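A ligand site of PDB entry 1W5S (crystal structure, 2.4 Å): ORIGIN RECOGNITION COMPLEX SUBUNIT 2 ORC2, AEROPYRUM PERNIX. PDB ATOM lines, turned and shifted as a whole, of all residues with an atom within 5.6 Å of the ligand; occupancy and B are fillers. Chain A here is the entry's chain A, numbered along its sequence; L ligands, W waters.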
ATOM      1  N   ASP A  16      34.402   1.666  16.584  1.00  0.00           N
ATOM      2  CA  ASP A  16      33.649   1.861  15.334  1.00  0.00           C
ATOM      3  C   ASP A  16      32.275   1.218  15.522  1.00  0.00           C
ATOM      4  O   ASP A  16      32.159   0.250  16.283  1.00  0.00           O
ATOM      5  CB  ASP A  16      34.361   1.300  14.083  1.00  0.00           C
ATOM      6  CG  ASP A  16      35.662   2.090  13.678  1.00  0.00           C
ATOM      7  OD1 ASP A  16      35.764   3.361  13.765  1.00  0.00           O
ATOM      8  OD2 ASP A  16      36.631   1.398  13.253  1.00  0.00           O
ATOM      9  N   GLU A  17      31.253   1.755  14.840  1.00  0.00           N
ATOM     10  CA  GLU A  17      29.891   1.191  14.841  1.00  0.00           C
ATOM     11  C   GLU A  17      29.851  -0.294  14.443  1.00  0.00           C
ATOM     12  O   GLU A  17      28.946  -1.016  14.826  1.00  0.00           O
ATOM     13  CB  GLU A  17      28.951   1.975  13.872  1.00  0.00           C
ATOM     14  CG  GLU A  17      28.652   3.520  14.194  1.00  0.00           C
ATOM     15  CD  GLU A  17      27.254   3.832  14.903  1.00  0.00           C
ATOM     16  OE1 GLU A  17      27.167   4.681  15.873  1.00  0.00           O
ATOM     17  OE2 GLU A  17      26.254   3.212  14.432  1.00  0.00           O
ATOM     18  N   TYR A  19      32.335  -2.750  14.878  1.00  0.00           N
ATOM     19  CA  TYR A  19      33.155  -3.631  15.687  1.00  0.00           C
ATOM     20  C   TYR A  19      32.330  -4.571  16.535  1.00  0.00           C
ATOM     21  O   TYR A  19      31.452  -4.141  17.244  1.00  0.00           O
ATOM     22  CB  TYR A  19      34.086  -2.833  16.616  1.00  0.00           C
ATOM     23  CG  TYR A  19      34.972  -3.656  17.547  1.00  0.00           C
ATOM     24  CD1 TYR A  19      36.202  -4.201  17.099  1.00  0.00           C
ATOM     25  CD2 TYR A  19      34.593  -3.891  18.857  1.00  0.00           C
ATOM     26  CE1 TYR A  19      37.017  -4.932  17.952  1.00  0.00           C
ATOM     27  CE2 TYR A  19      35.390  -4.626  19.722  1.00  0.00           C
ATOM     28  CZ  TYR A  19      36.605  -5.143  19.266  1.00  0.00           C
ATOM     29  OH  TYR A  19      37.404  -5.861  20.132  1.00  0.00           O
ATOM     30  N   ILE A  20      32.580  -5.871  16.414  1.00  0.00           N
ATOM     31  CA  ILE A  20      32.097  -6.835  17.392  1.00  0.00           C
ATOM     32  C   ILE A  20      33.324  -7.253  18.205  1.00  0.00           C
ATOM     33  O   ILE A  20      34.393  -7.475  17.660  1.00  0.00           O
ATOM     34  CB  ILE A  20      31.544  -8.106  16.770  1.00  0.00           C
ATOM     35  CG1 ILE A  20      30.739  -7.868  15.472  1.00  0.00           C
ATOM     36  CG2 ILE A  20      30.716  -8.839  17.817  1.00  0.00           C
ATOM     37  CD1 ILE A  20      29.311  -7.516  15.677  1.00  0.00           C
ATOM     38  N   PRO A  21      33.151  -7.375  19.526  1.00  0.00           N
ATOM     39  CA  PRO A  21      34.232  -7.901  20.346  1.00  0.00           C
ATOM     40  C   PRO A  21      34.437  -9.415  20.141  1.00  0.00           C
ATOM     41  O   PRO A  21      33.552 -10.137  19.632  1.00  0.00           O
ATOM     42  CB  PRO A  21      33.772  -7.596  21.800  1.00  0.00           C
ATOM     43  CG  PRO A  21      32.373  -7.254  21.722  1.00  0.00           C
ATOM     44  CD  PRO A  21      31.921  -7.190  20.295  1.00  0.00           C
ATOM     45  N   LEU A  24      31.291 -12.181  23.797  1.00  0.00           N
ATOM     46  CA  LEU A  24      30.188 -11.440  24.348  1.00  0.00           C
ATOM     47  C   LEU A  24      30.204 -11.605  25.859  1.00  0.00           C
ATOM     48  O   LEU A  24      30.598 -12.639  26.329  1.00  0.00           O
ATOM     49  CB  LEU A  24      28.853 -11.916  23.778  1.00  0.00           C
ATOM     50  CG  LEU A  24      28.612 -11.575  22.307  1.00  0.00           C
ATOM     51  CD1 LEU A  24      27.299 -12.112  21.909  1.00  0.00           C
ATOM     52  CD2 LEU A  24      28.674 -10.072  22.001  1.00  0.00           C
ATOM     53  N   ARG A  25      29.824 -10.567  26.611  1.00  0.00           N
ATOM     54  CA  ARG A  25      29.750 -10.684  28.054  1.00  0.00           C
ATOM     55  C   ARG A  25      28.357 -10.413  28.546  1.00  0.00           C
ATOM     56  O   ARG A  25      28.075 -10.551  29.756  1.00  0.00           O
ATOM     57  CB  ARG A  25      30.719  -9.731  28.755  1.00  0.00           C
ATOM     58  CG  ARG A  25      32.160 -10.084  28.545  1.00  0.00           C
ATOM     59  CD  ARG A  25      33.062  -9.083  29.253  1.00  0.00           C
ATOM     60  NE  ARG A  25      34.470  -9.398  29.076  1.00  0.00           N
ATOM     61  CZ  ARG A  25      35.484  -8.694  29.568  1.00  0.00           C
ATOM     62  NH1 ARG A  25      35.306  -7.554  30.263  1.00  0.00           N
ATOM     63  NH2 ARG A  25      36.712  -9.112  29.350  1.00  0.00           N
ATOM     64  N   VAL A  26      27.471 -10.041  27.638  1.00  0.00           N
ATOM     65  CA  VAL A  26      26.095  -9.762  28.019  1.00  0.00           C
ATOM     66  C   VAL A  26      25.084 -10.662  27.272  1.00  0.00           C
ATOM     67  O   VAL A  26      24.009 -10.995  27.825  1.00  0.00           O
ATOM     68  CB  VAL A  26      25.728  -8.265  27.854  1.00  0.00           C
ATOM     69  CG1 VAL A  26      24.244  -8.075  28.063  1.00  0.00           C
ATOM     70  CG2 VAL A  26      26.487  -7.401  28.869  1.00  0.00           C
ATOM     71  N   ARG A  27      25.356 -11.003  26.031  1.00  0.00           N
ATOM     72  CA  ARG A  27      24.363 -11.802  25.307  1.00  0.00           C
ATOM     73  C   ARG A  27      24.915 -13.224  25.103  1.00  0.00           C
ATOM     74  O   ARG A  27      24.507 -13.942  24.193  1.00  0.00           O
ATOM     75  CB  ARG A  27      24.127 -11.191  23.897  1.00  0.00           C
ATOM     76  CG  ARG A  27      23.432  -9.826  23.868  1.00  0.00           C
ATOM     77  CD  ARG A  27      22.066  -9.870  24.395  1.00  0.00           C
ATOM     78  NE  ARG A  27      21.271  -8.714  23.958  1.00  0.00           N
ATOM     79  CZ  ARG A  27      20.225  -8.251  24.658  1.00  0.00           C
ATOM     80  NH1 ARG A  27      19.915  -8.830  25.836  1.00  0.00           N
ATOM     81  NH2 ARG A  27      19.525  -7.185  24.223  1.00  0.00           N
ATOM     82  N   ARG A  60      12.837   0.420  19.923  1.00  0.00           N
ATOM     83  CA  ARG A  60      14.141   0.171  20.544  1.00  0.00           C
ATOM     84  C   ARG A  60      15.228  -0.050  19.492  1.00  0.00           C
ATOM     85  O   ARG A  60      15.005  -0.748  18.555  1.00  0.00           O
ATOM     86  CB  ARG A  60      14.051  -1.063  21.450  1.00  0.00           C
ATOM     87  CG  ARG A  60      13.096  -0.975  22.571  1.00  0.00           C
ATOM     88  CD  ARG A  60      13.422   0.176  23.494  1.00  0.00           C
ATOM     89  NE  ARG A  60      12.929  -0.151  24.825  1.00  0.00           N
ATOM     90  CZ  ARG A  60      12.720   0.709  25.814  1.00  0.00           C
ATOM     91  NH1 ARG A  60      12.296   0.254  26.968  1.00  0.00           N
ATOM     92  NH2 ARG A  60      12.979   1.999  25.675  1.00  0.00           N
ATOM     93  N   VAL A  61      16.384   0.622  19.646  1.00  0.00           N
ATOM     94  CA  VAL A  61      17.537   0.492  18.760  1.00  0.00           C
ATOM     95  C   VAL A  61      18.751   0.356  19.625  1.00  0.00           C
ATOM     96  O   VAL A  61      18.714   0.811  20.737  1.00  0.00           O
ATOM     97  CB  VAL A  61      17.733   1.711  17.797  1.00  0.00           C
ATOM     98  CG1 VAL A  61      16.481   1.973  17.056  1.00  0.00           C
ATOM     99  CG2 VAL A  61      18.046   2.961  18.574  1.00  0.00           C
ATOM    100  N   GLY A  62      19.798  -0.255  19.117  1.00  0.00           N
ATOM    101  CA  GLY A  62      21.087  -0.338  19.767  1.00  0.00           C
ATOM    102  C   GLY A  62      21.126  -1.351  20.885  1.00  0.00           C
ATOM    103  O   GLY A  62      21.962  -1.247  21.793  1.00  0.00           O
ATOM    104  N   ILE A  63      20.256  -2.355  20.784  1.00  0.00           N
ATOM    105  CA  ILE A  63      20.076  -3.347  21.813  1.00  0.00           C
ATOM    106  C   ILE A  63      20.796  -4.713  21.545  1.00  0.00           C
ATOM    107  O   ILE A  63      20.592  -5.693  22.306  1.00  0.00           O
ATOM    108  CB  ILE A  63      18.558  -3.584  22.061  1.00  0.00           C
ATOM    109  CG1 ILE A  63      17.888  -4.070  20.782  1.00  0.00           C
ATOM    110  CG2 ILE A  63      17.910  -2.256  22.539  1.00  0.00           C
ATOM    111  CD1 ILE A  63      16.517  -4.479  20.928  1.00  0.00           C
ATOM    112  N   GLY A  64      21.628  -4.759  20.487  1.00  0.00           N
ATOM    113  CA  GLY A  64      22.474  -5.909  20.237  1.00  0.00           C
ATOM    114  C   GLY A  64      21.873  -6.925  19.251  1.00  0.00           C
ATOM    115  O   GLY A  64      22.302  -8.053  19.182  1.00  0.00           O
ATOM    116  N   LYS A  65      20.882  -6.517  18.487  1.00  0.00           N
ATOM    117  CA  LYS A  65      20.274  -7.386  17.524  1.00  0.00           C
ATOM    118  C   LYS A  65      21.285  -7.812  16.498  1.00  0.00           C
ATOM    119  O   LYS A  65      21.607  -9.013  16.423  1.00  0.00           O
ATOM    120  CB  LYS A  65      19.080  -6.731  16.887  1.00  0.00           C
ATOM    121  CG  LYS A  65      17.896  -6.627  17.802  1.00  0.00           C
ATOM    122  CD  LYS A  65      16.639  -6.167  17.030  1.00  0.00           C
ATOM    123  CE  LYS A  65      16.847  -4.862  16.139  1.00  0.00           C
ATOM    124  NZ  LYS A  65      17.081  -3.623  17.011  1.00  0.00           N
ATOM    125  N   THR A  66      21.828  -6.840  15.759  1.00  0.00           N
ATOM    126  CA  THR A  66      22.857  -7.073  14.705  1.00  0.00           C
ATOM    127  C   THR A  66      24.039  -7.813  15.270  1.00  0.00           C
ATOM    128  O   THR A  66      24.489  -8.785  14.684  1.00  0.00           O
ATOM    129  CB  THR A  66      23.214  -5.735  14.033  1.00  0.00           C
ATOM    130  OG1 THR A  66      22.021  -5.312  13.411  1.00  0.00           O
ATOM    131  CG2 THR A  66      24.263  -5.791  12.885  1.00  0.00           C
ATOM    132  N   THR A  67      24.519  -7.392  16.430  1.00  0.00           N
ATOM    133  CA  THR A  67      25.665  -7.983  17.056  1.00  0.00           C
ATOM    134  C   THR A  67      25.435  -9.406  17.413  1.00  0.00           C
ATOM    135  O   THR A  67      26.290 -10.242  17.198  1.00  0.00           O
ATOM    136  CB  THR A  67      25.975  -7.187  18.356  1.00  0.00           C
ATOM    137  OG1 THR A  67      26.118  -5.800  18.048  1.00  0.00           O
ATOM    138  CG2 THR A  67      27.236  -7.654  18.993  1.00  0.00           C
ATOM    139  N   LEU A  68      24.272  -9.707  18.005  1.00  0.00           N
ATOM    140  CA  LEU A  68      23.917 -11.067  18.390  1.00  0.00           C
ATOM    141  C   LEU A  68      23.878 -11.904  17.164  1.00  0.00           C
ATOM    142  O   LEU A  68      24.311 -13.020  17.212  1.00  0.00           O
ATOM    143  CB  LEU A  68      22.580 -11.167  19.083  1.00  0.00           C
ATOM    144  CG  LEU A  68      22.307 -12.588  19.634  1.00  0.00           C
ATOM    145  CD1 LEU A  68      23.385 -12.993  20.627  1.00  0.00           C
ATOM    146  CD2 LEU A  68      20.993 -12.685  20.252  1.00  0.00           C
ATOM    147  N   ASP A 145      19.133  -8.558   7.868  1.00  0.00           N
ATOM    148  CA  ASP A 145      18.994  -7.520   8.885  1.00  0.00           C
ATOM    149  C   ASP A 145      18.010  -6.480   8.369  1.00  0.00           C
ATOM    150  O   ASP A 145      17.782  -6.392   7.179  1.00  0.00           O
ATOM    151  CB  ASP A 145      20.374  -6.900   9.192  1.00  0.00           C
ATOM    152  CG  ASP A 145      20.449  -6.275  10.603  1.00  0.00           C
ATOM    153  OD1 ASP A 145      19.413  -6.167  11.219  1.00  0.00           O
ATOM    154  OD2 ASP A 145      21.543  -5.871  11.046  1.00  0.00           O
ATOM    155  N   TYR A 215      18.883  -2.965  27.080  1.00  0.00           N
ATOM    156  CA  TYR A 215      19.899  -3.121  28.128  1.00  0.00           C
ATOM    157  C   TYR A 215      19.640  -2.367  29.410  1.00  0.00           C
ATOM    158  O   TYR A 215      19.247  -1.210  29.407  1.00  0.00           O
ATOM    159  CB  TYR A 215      21.289  -2.723  27.619  1.00  0.00           C
ATOM    160  CG  TYR A 215      21.801  -3.701  26.584  1.00  0.00           C
ATOM    161  CD1 TYR A 215      22.153  -3.269  25.302  1.00  0.00           C
ATOM    162  CD2 TYR A 215      21.935  -5.061  26.900  1.00  0.00           C
ATOM    163  CE1 TYR A 215      22.646  -4.147  24.370  1.00  0.00           C
ATOM    164  CE2 TYR A 215      22.397  -5.924  26.000  1.00  0.00           C
ATOM    165  CZ  TYR A 215      22.748  -5.479  24.712  1.00  0.00           C
ATOM    166  OH  TYR A 215      23.217  -6.390  23.810  1.00  0.00           O
ATOM    167  N   ILE A 223      29.153  -3.811  29.053  1.00  0.00           N
ATOM    168  CA  ILE A 223      29.506  -3.527  27.641  1.00  0.00           C
ATOM    169  C   ILE A 223      30.542  -2.440  27.516  1.00  0.00           C
ATOM    170  O   ILE A 223      31.430  -2.564  26.733  1.00  0.00           O
ATOM    171  CB  ILE A 223      28.227  -3.132  26.804  1.00  0.00           C
ATOM    172  CG1 ILE A 223      27.415  -4.411  26.551  1.00  0.00           C
ATOM    173  CG2 ILE A 223      28.537  -2.412  25.499  1.00  0.00           C
ATOM    174  CD1 ILE A 223      26.022  -4.166  26.038  1.00  0.00           C
ATOM    175  N   GLN A 226      34.107  -3.459  28.742  1.00  0.00           N
ATOM    176  CA  GLN A 226      34.838  -4.370  27.859  1.00  0.00           C
ATOM    177  C   GLN A 226      35.486  -3.552  26.718  1.00  0.00           C
ATOM    178  O   GLN A 226      36.610  -3.827  26.249  1.00  0.00           O
ATOM    179  CB  GLN A 226      33.891  -5.454  27.318  1.00  0.00           C
ATOM    180  CG  GLN A 226      34.410  -6.180  26.091  1.00  0.00           C
ATOM    181  CD  GLN A 226      33.454  -7.229  25.572  1.00  0.00           C
ATOM    182  OE1 GLN A 226      32.272  -6.934  25.288  1.00  0.00           O
ATOM    183  NE2 GLN A 226      33.967  -8.452  25.403  1.00  0.00           N
ATOM    184  N   ARG A 227      34.748  -2.536  26.267  1.00  0.00           N
ATOM    185  CA  ARG A 227      35.272  -1.619  25.257  1.00  0.00           C
ATOM    186  C   ARG A 227      36.433  -0.797  25.836  1.00  0.00           C
ATOM    187  O   ARG A 227      37.405  -0.504  25.157  1.00  0.00           O
ATOM    188  CB  ARG A 227      34.171  -0.669  24.811  1.00  0.00           C
ATOM    189  CG  ARG A 227      33.047  -1.337  24.168  1.00  0.00           C
ATOM    190  CD  ARG A 227      33.415  -2.043  22.905  1.00  0.00           C
ATOM    191  NE  ARG A 227      32.252  -2.735  22.405  1.00  0.00           N
ATOM    192  CZ  ARG A 227      31.693  -2.532  21.229  1.00  0.00           C
ATOM    193  NH1 ARG A 227      32.247  -1.768  20.350  1.00  0.00           N
ATOM    194  NH2 ARG A 227      30.629  -3.229  20.894  1.00  0.00           N
ATOM    195  N   ALA A 259      22.959   0.404  23.653  1.00  0.00           N
ATOM    196  CA  ALA A 259      24.392   0.221  23.789  1.00  0.00           C
ATOM    197  C   ALA A 259      25.140   1.102  22.775  1.00  0.00           C
ATOM    198  O   ALA A 259      26.251   1.520  23.027  1.00  0.00           O
ATOM    199  CB  ALA A 259      24.787  -1.263  23.621  1.00  0.00           C
ATOM    200  N   ARG A 260      24.501   1.427  21.658  1.00  0.00           N
ATOM    201  CA  ARG A 260      25.087   2.311  20.698  1.00  0.00           C
ATOM    202  C   ARG A 260      25.216   3.716  21.271  1.00  0.00           C
ATOM    203  O   ARG A 260      26.306   4.280  21.192  1.00  0.00           O
ATOM    204  CB  ARG A 260      24.306   2.335  19.370  1.00  0.00           C
ATOM    205  CG  ARG A 260      24.709   3.507  18.479  1.00  0.00           C
ATOM    206  CD  ARG A 260      24.477   3.294  17.033  1.00  0.00           C
ATOM    207  NE  ARG A 260      23.344   2.370  16.882  1.00  0.00           N
ATOM    208  CZ  ARG A 260      23.344   1.203  16.215  1.00  0.00           C
ATOM    209  NH1 ARG A 260      24.410   0.730  15.510  1.00  0.00           N
ATOM    210  NH2 ARG A 260      22.201   0.517  16.249  1.00  0.00           N
ATOM    211  N   ILE A 263      28.106   3.595  23.919  1.00  0.00           N
ATOM    212  CA  ILE A 263      29.484   3.500  23.399  1.00  0.00           C
ATOM    213  C   ILE A 263      29.902   4.837  22.686  1.00  0.00           C
ATOM    214  O   ILE A 263      31.011   5.315  22.856  1.00  0.00           O
ATOM    215  CB  ILE A 263      29.667   2.265  22.505  1.00  0.00           C
ATOM    216  CG1 ILE A 263      29.705   1.026  23.388  1.00  0.00           C
ATOM    217  CG2 ILE A 263      30.952   2.351  21.560  1.00  0.00           C
ATOM    218  CD1 ILE A 263      29.414  -0.237  22.707  1.00  0.00           C
HETATM  219  P1  LIG L   1      20.617  -3.062  17.226  1.00  0.00           P
HETATM  220  O1  LIG L   1      20.315  -1.649  16.802  1.00  0.00           O
HETATM  221  O2  LIG L   1      19.532  -3.665  18.106  1.00  0.00           O
HETATM  222  O3  LIG L   1      20.910  -3.958  16.005  1.00  0.00           O
HETATM  223  P2  LIG L   1      23.511  -3.301  17.539  1.00  0.00           P
HETATM  224  O4  LIG L   1      23.679  -2.473  16.319  1.00  0.00           O
HETATM  225  O5  LIG L   1      23.731  -4.797  17.552  1.00  0.00           O
HETATM  226  O6  LIG L   1      21.969  -2.972  18.098  1.00  0.00           O
HETATM  227  O7  LIG L   1      24.393  -2.649  18.746  1.00  0.00           O
HETATM  228  C1  LIG L   1      24.581  -1.234  18.948  1.00  0.00           C
HETATM  229  C2  LIG L   1      25.972  -0.986  19.440  1.00  0.00           C
HETATM  230  O8  LIG L   1      26.142  -1.586  20.741  1.00  0.00           O
HETATM  231  C3  LIG L   1      27.045  -1.616  18.569  1.00  0.00           C
HETATM  232  O9  LIG L   1      28.258  -0.893  18.692  1.00  0.00           O
HETATM  233  C4  LIG L   1      27.283  -3.005  19.186  1.00  0.00           C
HETATM  234  O10 LIG L   1      28.637  -3.496  18.983  1.00  0.00           O
HETATM  235  C5  LIG L   1      27.073  -2.682  20.679  1.00  0.00           C
HETATM  236  N1  LIG L   1      26.624  -3.899  21.381  1.00  0.00           N
HETATM  237  C6  LIG L   1      25.335  -4.293  21.440  1.00  0.00           C
HETATM  238  N2  LIG L   1      25.202  -5.405  22.139  1.00  0.00           N
HETATM  239  C7  LIG L   1      26.401  -5.741  22.574  1.00  0.00           C
HETATM  240  C8  LIG L   1      26.905  -6.867  23.362  1.00  0.00           C
HETATM  241  N3  LIG L   1      26.010  -7.796  23.792  1.00  0.00           N
HETATM  242  N4  LIG L   1      28.230  -6.906  23.634  1.00  0.00           N
HETATM  243  C9  LIG L   1      29.065  -5.929  23.133  1.00  0.00           C
HETATM  244  N5  LIG L   1      28.623  -4.895  22.377  1.00  0.00           N
HETATM  245  C10 LIG L   1      27.350  -4.740  22.078  1.00  0.00           C
HETATM  246  O   HOH W   1      30.799  -1.432  18.050  1.00  0.00           O
HETATM  247  O   HOH W   2      31.587  -4.321  24.435  1.00  0.00           O
HETATM  248  O   HOH W   3      29.928  -8.080  25.411  1.00  0.00           O
HETATM  249  O   HOH W   4      19.178  -4.239  13.301  1.00  0.00           O
HETATM  250  O   HOH W   5      22.889  -2.365  13.768  1.00  0.00           O
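Glu 17 touches the ligand.
Pro 21 touches the ligand.
Leu 24 touches the ligand.
CG of Arg 27 touches N3 of the ligand (3.3 Å).
C of Val 61 touches O1 of the ligand, 3.8 Å away.
Ile 223 touches the ligand (CD1 to C7, 3.8 Å).
Gln 226 touches the ligand (OE1 to C9, 3.99 Å).
Ala 259 touches the ligand.
CD1 of Ile 263 touches C5 of the ligand, 3.9 Å away.
Hydrophobic or aromatic side chains that line the ligand: Pro 21, Leu 24, Ile 63, Tyr 215, Ile 223, Ala 259 and Ile 263.
19 residues have an atom within 4 Å of the ligand: Glu 17, Tyr 19, Pro 21, Leu 24, Arg 27, Val 61, Gly 62, Ile 63, Gly 64, Lys 65, Thr 66, Thr 67, Tyr 215, Ile 223, Gln 226, Arg 227, Ala 259, Arg 260 and Ile 263.
An oxygen (O5) of the ligand sits at hydrogen-bond distance from the backbone NH (N) of Thr 67.
O5 of the ligand lies within hydrogen-bond range of OG1 of Thr 67 (2.6 Å).
N of Lys 65 lies within hydrogen-bond range of O2 of the ligand, 3.2 Å away.
The side-chain amino group (NZ) of Lys 65 is in salt-bridge range of an oxygen (O2) of the ligand, at 2.7 Å.
An oxygen (O1) of the ligand lies within hydrogen-bond range of the backbone NH (N) of Gly 62 (2.8 Å).
The guanidinium group (NH2) of Arg 227 is in hydrogen-bond range of an oxygen (O10) of the ligand, at 2.8 Å.
The side-chain hydroxyl (OH) of Tyr 215 lies within hydrogen-bond range of a nitrogen (N2) of the ligand (2.8 Å).
The guanidinium group (NH2) of Arg 260 is in salt-bridge range of an oxygen (O1) of the ligand.
An oxygen (O6) of the ligand sits at hydrogen-bond distance from the backbone NH of Gly 64 (3.0 Å).
O3 of the ligand sits at hydrogen-bond distance from N of Thr 66.
OG1 of Thr 66 is in hydrogen-bond range of O3 of the ligand (3.1 Å).
O2 of the ligand lies within hydrogen-bond range of N of Ile 63 (3.1 Å).
O10 of the ligand sits at hydrogen-bond distance from O of Tyr 19, 3.4 Å away.
Water W5 lies within hydrogen-bond range of O4 of the ligand and OG1 of Thr 66.
Water W1 lies within hydrogen-bond range of an oxygen (O9) of the ligand (2.7 Å), the guanidinium group of Arg 227 (2.7 Å), the backbone carbonyl oxygen of Asp 16 (2.8 Å) and the backbone carbonyl oxygen of Tyr 19 (2.9 Å).
Water W3 lies within hydrogen-bond range of OE1 of Gln 226, N4 of the ligand and N of Arg 25.
Water W4 lies within hydrogen-bond range of the side-chain carboxylate of Asp 145 (2.8 Å), the side-chain hydroxyl of Thr 66 (3.0 Å) and an oxygen (O3) of the ligand (3.2 Å).
Water W2 lies within hydrogen-bond range of the guanidinium group (NE) of Arg 227 (2.7 Å), the side-chain amide oxygen (OE1) of Gln 226 (2.8 Å) and the backbone carbonyl oxygen (O) of Ile 223 (2.9 Å).
The backbone carbonyl oxygen of Gly 62 sits at hydrogen-bond distance from the backbone NH of Ala 259 (2.7 Å).
The side-chain hydroxyl (OH) of Tyr 215 lies within hydrogen-bond range of the backbone carbonyl oxygen (O) of Ile 63 (3.1 Å).
OH of Tyr 215 is in hydrogen-bond range of NE of Arg 27, at 3.0 Å.
The side-chain carboxylate (OE2) of Glu 17 is in salt-bridge range of the guanidinium group (NH1) of Arg 260 (3.3 Å).
OG1 of Thr 66 lies within hydrogen-bond range of OD2 of Asp 145 (2.5 Å).
O of Ile 63 lies within hydrogen-bond range of NH2 of Arg 27, 2.7 Å away.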
